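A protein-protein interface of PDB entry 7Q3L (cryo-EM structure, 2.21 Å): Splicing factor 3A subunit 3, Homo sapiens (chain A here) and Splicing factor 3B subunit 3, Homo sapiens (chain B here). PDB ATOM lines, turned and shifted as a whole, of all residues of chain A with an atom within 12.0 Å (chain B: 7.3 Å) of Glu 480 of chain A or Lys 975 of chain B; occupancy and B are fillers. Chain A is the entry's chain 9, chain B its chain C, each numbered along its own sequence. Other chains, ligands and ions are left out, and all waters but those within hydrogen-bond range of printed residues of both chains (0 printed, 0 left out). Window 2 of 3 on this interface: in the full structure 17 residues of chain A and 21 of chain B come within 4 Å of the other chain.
ND1 of His 941 of chain B lies within hydrogen-bond range of O of Lys 974 of chain B (3.0 Å).
OG1 of Thr 943 of chain B sits at hydrogen-bond distance from N of Leu 977 of chain B, at 3.3 Å.
The backbone NH (N) of Glu 478 of chain A lies within hydrogen-bond range of the backbone carbonyl oxygen (O) of Val 487 of chain A, at 2.8 Å.
The side-chain carboxylate (OE2) of Glu 480 of chain A sits at hydrogen-bond distance from the side-chain hydroxyl (OH) of Tyr 479 of chain A, at 2.8 Å.
Of the 11 printed residues of chain B, 5 touch a printed residue of chain A.
Printed residues of chain B that touch a printed residue of chain A: Lys 974, Lys 975, Lys 976, Leu 977 and Leu 978.
Of the 8 printed residues of chain A, 5 touch a printed residue of chain B.
Hydrophobic or aromatic side chains of chain A that line the printed part of chain B: Tyr 479 and Val 486.
Along chain A the printed residues that touch a printed residue of chain B span positions 477 to 486.
Glu 480 of chain A touches just one residue of chain B: Lys 975.
Of chain A, only Tyr 479 (3.2 Å) and Glu 480 (3.4 Å) come within 4 Å of Lys 975 of chain B.
No residue of chain A comes within 4 Å of Gly 973 of chain B.
Of chain A, only Tyr 479 (3.4 Å) comes within 4 Å of Lys 974 of chain B.
Printed residues of chain A within 4 Å of Lys 976 of chain B: Glu 477 (3.1 Å) and Val 486 (3.8 Å).
Of the printed residues of chain B, Tyr 479 of chain A touches Lys 974, Lys 975 and Leu 978.
Printed residues of chain B within 4 Å of Glu 477 of chain A: Lys 976, Leu 977 and Leu 978.
Printed residues of chain B within 4 Å of Glu 478 of chain A: Leu 978 (3.9 Å).
Of the printed residues of chain A, Leu 978 of chain B touches Glu 477, Glu 478 and Tyr 479.
Printed residues of chain A within 4 Å of Leu 977 of chain B: Glu 477.
Leu 940 of chain B touches none of the printed residues of chain A.
The nearest printed residue of chain A that does not touch Leu 977 of chain B is Val 486 of chain A (6.3 Å).
The backbone NH of Lys 975 of chain B lies close to the side-chain hydroxyl of Tyr 479 of chain A, 3.3 Å away.
The side-chain amino group (NZ) of Lys 975 of chain B lies within salt-bridge range of the side-chain carboxylate (OE1) of Glu 480 of chain A, at 3.4 Å.
The side-chain carboxylate of Glu 477 of chain A is in salt-bridge range of the side-chain amino group of Lys 976 of chain B.
The side-chain carboxylate (OE1) of Glu 477 of chain A lies close to the backbone carbonyl oxygen (O) of Leu 977 of chain B (3.4 Å).
Among the printed residues, pairs that only touch across the chains: Tyr 479 of chain A with Lys 974 of chain B (3.4 Å), Glu 477 of chain A with Leu 978 of chain B (3.6 Å), Tyr 479 of chain A with Leu 978 of chain B (3.7 Å), Val 486 of chain A with Lys 976 of chain B (3.8 Å) and Glu 478 of chain A with Leu 978 of chain B (3.9 Å).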
ATOM      1  N   GLU A 476      21.300  19.608   8.562  1.00  0.00           N
ATOM      2  CA  GLU A 476      21.905  18.473   9.253  1.00  0.00           C
ATOM      3  C   GLU A 476      21.937  18.748  10.763  1.00  0.00           C
ATOM      4  O   GLU A 476      22.070  19.892  11.183  1.00  0.00           O
ATOM      5  CB  GLU A 476      23.310  18.252   8.687  1.00  0.00           C
ATOM      6  CG  GLU A 476      24.046  17.070   9.293  1.00  0.00           C
ATOM      7  CD  GLU A 476      25.273  16.572   8.548  1.00  0.00           C
ATOM      8  OE1 GLU A 476      25.376  16.808   7.323  1.00  0.00           O
ATOM      9  OE2 GLU A 476      26.104  15.904   9.182  1.00  0.00           O
ATOM     10  N   GLU A 477      21.830  17.702  11.593  1.00  0.00           N
ATOM     11  CA  GLU A 477      21.815  17.872  13.045  1.00  0.00           C
ATOM     12  C   GLU A 477      23.136  17.462  13.700  1.00  0.00           C
ATOM     13  O   GLU A 477      23.699  16.407  13.403  1.00  0.00           O
ATOM     14  CB  GLU A 477      20.642  17.124  13.677  1.00  0.00           C
ATOM     15  CG  GLU A 477      19.296  17.549  13.117  1.00  0.00           C
ATOM     16  CD  GLU A 477      18.105  17.065  13.929  1.00  0.00           C
ATOM     17  OE1 GLU A 477      18.083  15.885  14.321  1.00  0.00           O
ATOM     18  OE2 GLU A 477      17.192  17.880  14.176  1.00  0.00           O
ATOM     19  N   GLU A 478      23.593  18.301  14.648  1.00  0.00           N
ATOM     20  CA  GLU A 478      24.801  18.110  15.443  1.00  0.00           C
ATOM     21  C   GLU A 478      24.465  18.052  16.938  1.00  0.00           C
ATOM     22  O   GLU A 478      23.490  18.652  17.396  1.00  0.00           O
ATOM     23  CB  GLU A 478      25.807  19.235  15.175  1.00  0.00           C
ATOM     24  CG  GLU A 478      26.363  19.286  13.757  1.00  0.00           C
ATOM     25  CD  GLU A 478      27.116  18.053  13.286  1.00  0.00           C
ATOM     26  OE1 GLU A 478      27.518  18.023  12.111  1.00  0.00           O
ATOM     27  OE2 GLU A 478      27.239  17.093  14.074  1.00  0.00           O
ATOM     28  N   TYR A 479      25.286  17.317  17.705  1.00  0.00           N
ATOM     29  CA  TYR A 479      25.004  17.117  19.127  1.00  0.00           C
ATOM     30  C   TYR A 479      25.199  18.414  19.941  1.00  0.00           C
ATOM     31  O   TYR A 479      25.920  19.299  19.498  1.00  0.00           O
ATOM     32  CB  TYR A 479      25.416  15.715  19.652  1.00  0.00           C
ATOM     33  CG  TYR A 479      24.684  15.505  20.950  1.00  0.00           C
ATOM     34  CD1 TYR A 479      23.318  15.244  20.939  1.00  0.00           C
ATOM     35  CD2 TYR A 479      25.303  15.733  22.173  1.00  0.00           C
ATOM     36  CE1 TYR A 479      22.571  15.256  22.104  1.00  0.00           C
ATOM     37  CE2 TYR A 479      24.568  15.725  23.355  1.00  0.00           C
ATOM     38  CZ  TYR A 479      23.197  15.529  23.313  1.00  0.00           C
ATOM     39  OH  TYR A 479      22.492  15.616  24.485  1.00  0.00           O
ATOM     40  N   GLU A 480      24.558  18.498  21.128  1.00  0.00           N
ATOM     41  CA  GLU A 480      24.602  19.549  22.150  1.00  0.00           C
ATOM     42  C   GLU A 480      26.037  19.704  22.685  1.00  0.00           C
ATOM     43  O   GLU A 480      26.558  18.746  23.312  1.00  0.00           O
ATOM     44  CB  GLU A 480      23.567  19.104  23.197  1.00  0.00           C
ATOM     45  CG  GLU A 480      23.326  19.965  24.412  1.00  0.00           C
ATOM     46  CD  GLU A 480      22.350  19.254  25.341  1.00  0.00           C
ATOM     47  OE1 GLU A 480      21.338  19.884  25.706  1.00  0.00           O
ATOM     48  OE2 GLU A 480      22.591  18.079  25.711  1.00  0.00           O
ATOM     49  N   VAL A 486      21.354  20.615  21.048  1.00  0.00           N
ATOM     50  CA  VAL A 486      21.514  20.208  19.615  1.00  0.00           C
ATOM     51  C   VAL A 486      21.711  21.474  18.792  1.00  0.00           C
ATOM     52  O   VAL A 486      21.229  22.540  19.178  1.00  0.00           O
ATOM     53  CB  VAL A 486      20.311  19.363  19.146  1.00  0.00           C
ATOM     54  CG1 VAL A 486      20.179  19.249  17.630  1.00  0.00           C
ATOM     55  CG2 VAL A 486      20.402  17.983  19.750  1.00  0.00           C
ATOM     56  N   VAL A 487      22.481  21.352  17.704  1.00  0.00           N
ATOM     57  CA  VAL A 487      22.807  22.451  16.795  1.00  0.00           C
ATOM     58  C   VAL A 487      22.484  22.011  15.361  1.00  0.00           C
ATOM     59  O   VAL A 487      22.486  20.808  15.099  1.00  0.00           O
ATOM     60  CB  VAL A 487      24.290  22.862  16.956  1.00  0.00           C
ATOM     61  CG1 VAL A 487      24.683  24.061  16.097  1.00  0.00           C
ATOM     62  CG2 VAL A 487      24.672  23.096  18.417  1.00  0.00           C
ATOM     63  N   ASN A 488      22.088  22.961  14.497  1.00  0.00           N
ATOM     64  CA  ASN A 488      22.129  22.789  13.053  1.00  0.00           C
ATOM     65  C   ASN A 488      23.071  23.883  12.522  1.00  0.00           C
ATOM     66  O   ASN A 488      22.778  25.054  12.816  1.00  0.00           O
ATOM     67  CB  ASN A 488      20.728  22.780  12.393  1.00  0.00           C
ATOM     68  CG  ASN A 488      19.776  21.636  12.739  1.00  0.00           C
ATOM     69  OD1 ASN A 488      18.776  21.405  12.057  1.00  0.00           O
ATOM     70  ND2 ASN A 488      20.040  20.919  13.817  1.00  0.00           N
ATOM     71  N   LEU B 940      16.424   5.007  26.699  1.00  0.00           N
ATOM     72  CA  LEU B 940      17.449   6.021  26.525  1.00  0.00           C
ATOM     73  C   LEU B 940      16.832   7.383  26.193  1.00  0.00           C
ATOM     74  O   LEU B 940      17.065   8.346  26.923  1.00  0.00           O
ATOM     75  CB  LEU B 940      18.431   5.540  25.454  1.00  0.00           C
ATOM     76  CG  LEU B 940      19.682   6.397  25.293  1.00  0.00           C
ATOM     77  CD1 LEU B 940      20.661   6.185  26.445  1.00  0.00           C
ATOM     78  CD2 LEU B 940      20.376   6.087  23.974  1.00  0.00           C
ATOM     79  N   HIS B 941      16.069   7.459  25.093  1.00  0.00           N
ATOM     80  CA  HIS B 941      15.340   8.667  24.734  1.00  0.00           C
ATOM     81  C   HIS B 941      14.240   8.382  23.703  1.00  0.00           C
ATOM     82  O   HIS B 941      14.246   7.345  23.043  1.00  0.00           O
ATOM     83  CB  HIS B 941      16.344   9.764  24.330  1.00  0.00           C
ATOM     84  CG  HIS B 941      17.298   9.379  23.244  1.00  0.00           C
ATOM     85  ND1 HIS B 941      18.674   9.397  23.380  1.00  0.00           N
ATOM     86  CD2 HIS B 941      17.061   9.007  21.968  1.00  0.00           C
ATOM     87  CE1 HIS B 941      19.229   9.048  22.227  1.00  0.00           C
ATOM     88  NE2 HIS B 941      18.262   8.805  21.340  1.00  0.00           N
ATOM     89  N   LYS B 942      13.279   9.314  23.588  1.00  0.00           N
ATOM     90  CA  LYS B 942      12.161   9.249  22.659  1.00  0.00           C
ATOM     91  C   LYS B 942      12.236  10.454  21.720  1.00  0.00           C
ATOM     92  O   LYS B 942      12.137  11.591  22.173  1.00  0.00           O
ATOM     93  CB  LYS B 942      10.868   9.233  23.483  1.00  0.00           C
ATOM     94  CG  LYS B 942       9.550   9.245  22.722  1.00  0.00           C
ATOM     95  CD  LYS B 942       8.385   9.164  23.681  1.00  0.00           C
ATOM     96  CE  LYS B 942       7.059   9.138  22.957  1.00  0.00           C
ATOM     97  NZ  LYS B 942       5.924   8.722  23.808  1.00  0.00           N
ATOM     98  N   THR B 943      12.420  10.202  20.418  1.00  0.00           N
ATOM     99  CA  THR B 943      12.704  11.245  19.441  1.00  0.00           C
ATOM    100  C   THR B 943      11.476  11.452  18.556  1.00  0.00           C
ATOM    101  O   THR B 943      11.055  10.504  17.905  1.00  0.00           O
ATOM    102  CB  THR B 943      13.902  10.848  18.568  1.00  0.00           C
ATOM    103  OG1 THR B 943      15.031  10.598  19.401  1.00  0.00           O
ATOM    104  CG2 THR B 943      14.286  11.901  17.552  1.00  0.00           C
ATOM    105  N   LEU B 972      23.076   8.226  16.549  1.00  0.00           N
ATOM    106  CA  LEU B 972      22.474   7.948  17.849  1.00  0.00           C
ATOM    107  C   LEU B 972      22.234   9.225  18.658  1.00  0.00           C
ATOM    108  O   LEU B 972      21.149   9.400  19.223  1.00  0.00           O
ATOM    109  CB  LEU B 972      23.341   6.957  18.629  1.00  0.00           C
ATOM    110  CG  LEU B 972      22.899   6.675  20.063  1.00  0.00           C
ATOM    111  CD1 LEU B 972      21.637   5.827  20.099  1.00  0.00           C
ATOM    112  CD2 LEU B 972      24.009   5.992  20.836  1.00  0.00           C
ATOM    113  N   GLY B 973      23.248  10.104  18.728  1.00  0.00           N
ATOM    114  CA  GLY B 973      23.183  11.300  19.565  1.00  0.00           C
ATOM    115  C   GLY B 973      23.247  10.910  21.038  1.00  0.00           C
ATOM    116  O   GLY B 973      23.641   9.774  21.332  1.00  0.00           O
ATOM    117  N   LYS B 974      22.904  11.844  21.946  1.00  0.00           N
ATOM    118  CA  LYS B 974      22.864  11.503  23.364  1.00  0.00           C
ATOM    119  C   LYS B 974      21.463  11.687  23.949  1.00  0.00           C
ATOM    120  O   LYS B 974      20.971  10.805  24.655  1.00  0.00           O
ATOM    121  CB  LYS B 974      23.949  12.229  24.166  1.00  0.00           C
ATOM    122  CG  LYS B 974      25.390  11.914  23.797  1.00  0.00           C
ATOM    123  CD  LYS B 974      25.768  10.469  24.062  1.00  0.00           C
ATOM    124  CE  LYS B 974      26.983  10.010  23.285  1.00  0.00           C
ATOM    125  NZ  LYS B 974      26.735   9.967  21.824  1.00  0.00           N
ATOM    126  N   LYS B 975      20.848  12.848  23.672  1.00  0.00           N
ATOM    127  CA  LYS B 975      19.486  13.136  24.106  1.00  0.00           C
ATOM    128  C   LYS B 975      18.454  12.866  23.006  1.00  0.00           C
ATOM    129  O   LYS B 975      17.268  12.715  23.310  1.00  0.00           O
ATOM    130  CB  LYS B 975      19.346  14.566  24.645  1.00  0.00           C
ATOM    131  CG  LYS B 975      19.797  14.777  26.083  1.00  0.00           C
ATOM    132  CD  LYS B 975      19.678  16.220  26.532  1.00  0.00           C
ATOM    133  CE  LYS B 975      20.241  16.466  27.915  1.00  0.00           C
ATOM    134  NZ  LYS B 975      20.191  17.902  28.273  1.00  0.00           N
ATOM    135  N   LYS B 976      18.892  12.840  21.737  1.00  0.00           N
ATOM    136  CA  LYS B 976      17.997  12.545  20.617  1.00  0.00           C
ATOM    137  C   LYS B 976      18.789  12.050  19.406  1.00  0.00           C
ATOM    138  O   LYS B 976      19.988  12.297  19.343  1.00  0.00           O
ATOM    139  CB  LYS B 976      17.142  13.764  20.246  1.00  0.00           C
ATOM    140  CG  LYS B 976      17.819  14.823  19.389  1.00  0.00           C
ATOM    141  CD  LYS B 976      16.844  15.811  18.796  1.00  0.00           C
ATOM    142  CE  LYS B 976      17.454  16.662  17.702  1.00  0.00           C
ATOM    143  NZ  LYS B 976      16.481  17.635  17.148  1.00  0.00           N
ATOM    144  N   LEU B 977      18.112  11.384  18.451  1.00  0.00           N
ATOM    145  CA  LEU B 977      18.758  10.972  17.206  1.00  0.00           C
ATOM    146  C   LEU B 977      19.044  12.209  16.351  1.00  0.00           C
ATOM    147  O   LEU B 977      18.240  13.139  16.373  1.00  0.00           O
ATOM    148  CB  LEU B 977      17.845   9.999  16.450  1.00  0.00           C
ATOM    149  CG  LEU B 977      17.442   8.727  17.198  1.00  0.00           C
ATOM    150  CD1 LEU B 977      16.375   7.964  16.430  1.00  0.00           C
ATOM    151  CD2 LEU B 977      18.646   7.837  17.461  1.00  0.00           C
ATOM    152  N   LEU B 978      20.173  12.217  15.615  1.00  0.00           N
ATOM    153  CA  LEU B 978      20.565  13.373  14.811  1.00  0.00           C
ATOM    154  C   LEU B 978      20.424  13.040  13.328  1.00  0.00           C
ATOM    155  O   LEU B 978      20.973  12.032  12.901  1.00  0.00           O
ATOM    156  CB  LEU B 978      22.022  13.735  15.130  1.00  0.00           C
ATOM    157  CG  LEU B 978      22.352  13.949  16.605  1.00  0.00           C
ATOM    158  CD1 LEU B 978      23.857  14.006  16.802  1.00  0.00           C
ATOM    159  CD2 LEU B 978      21.673  15.207  17.135  1.00  0.00           C
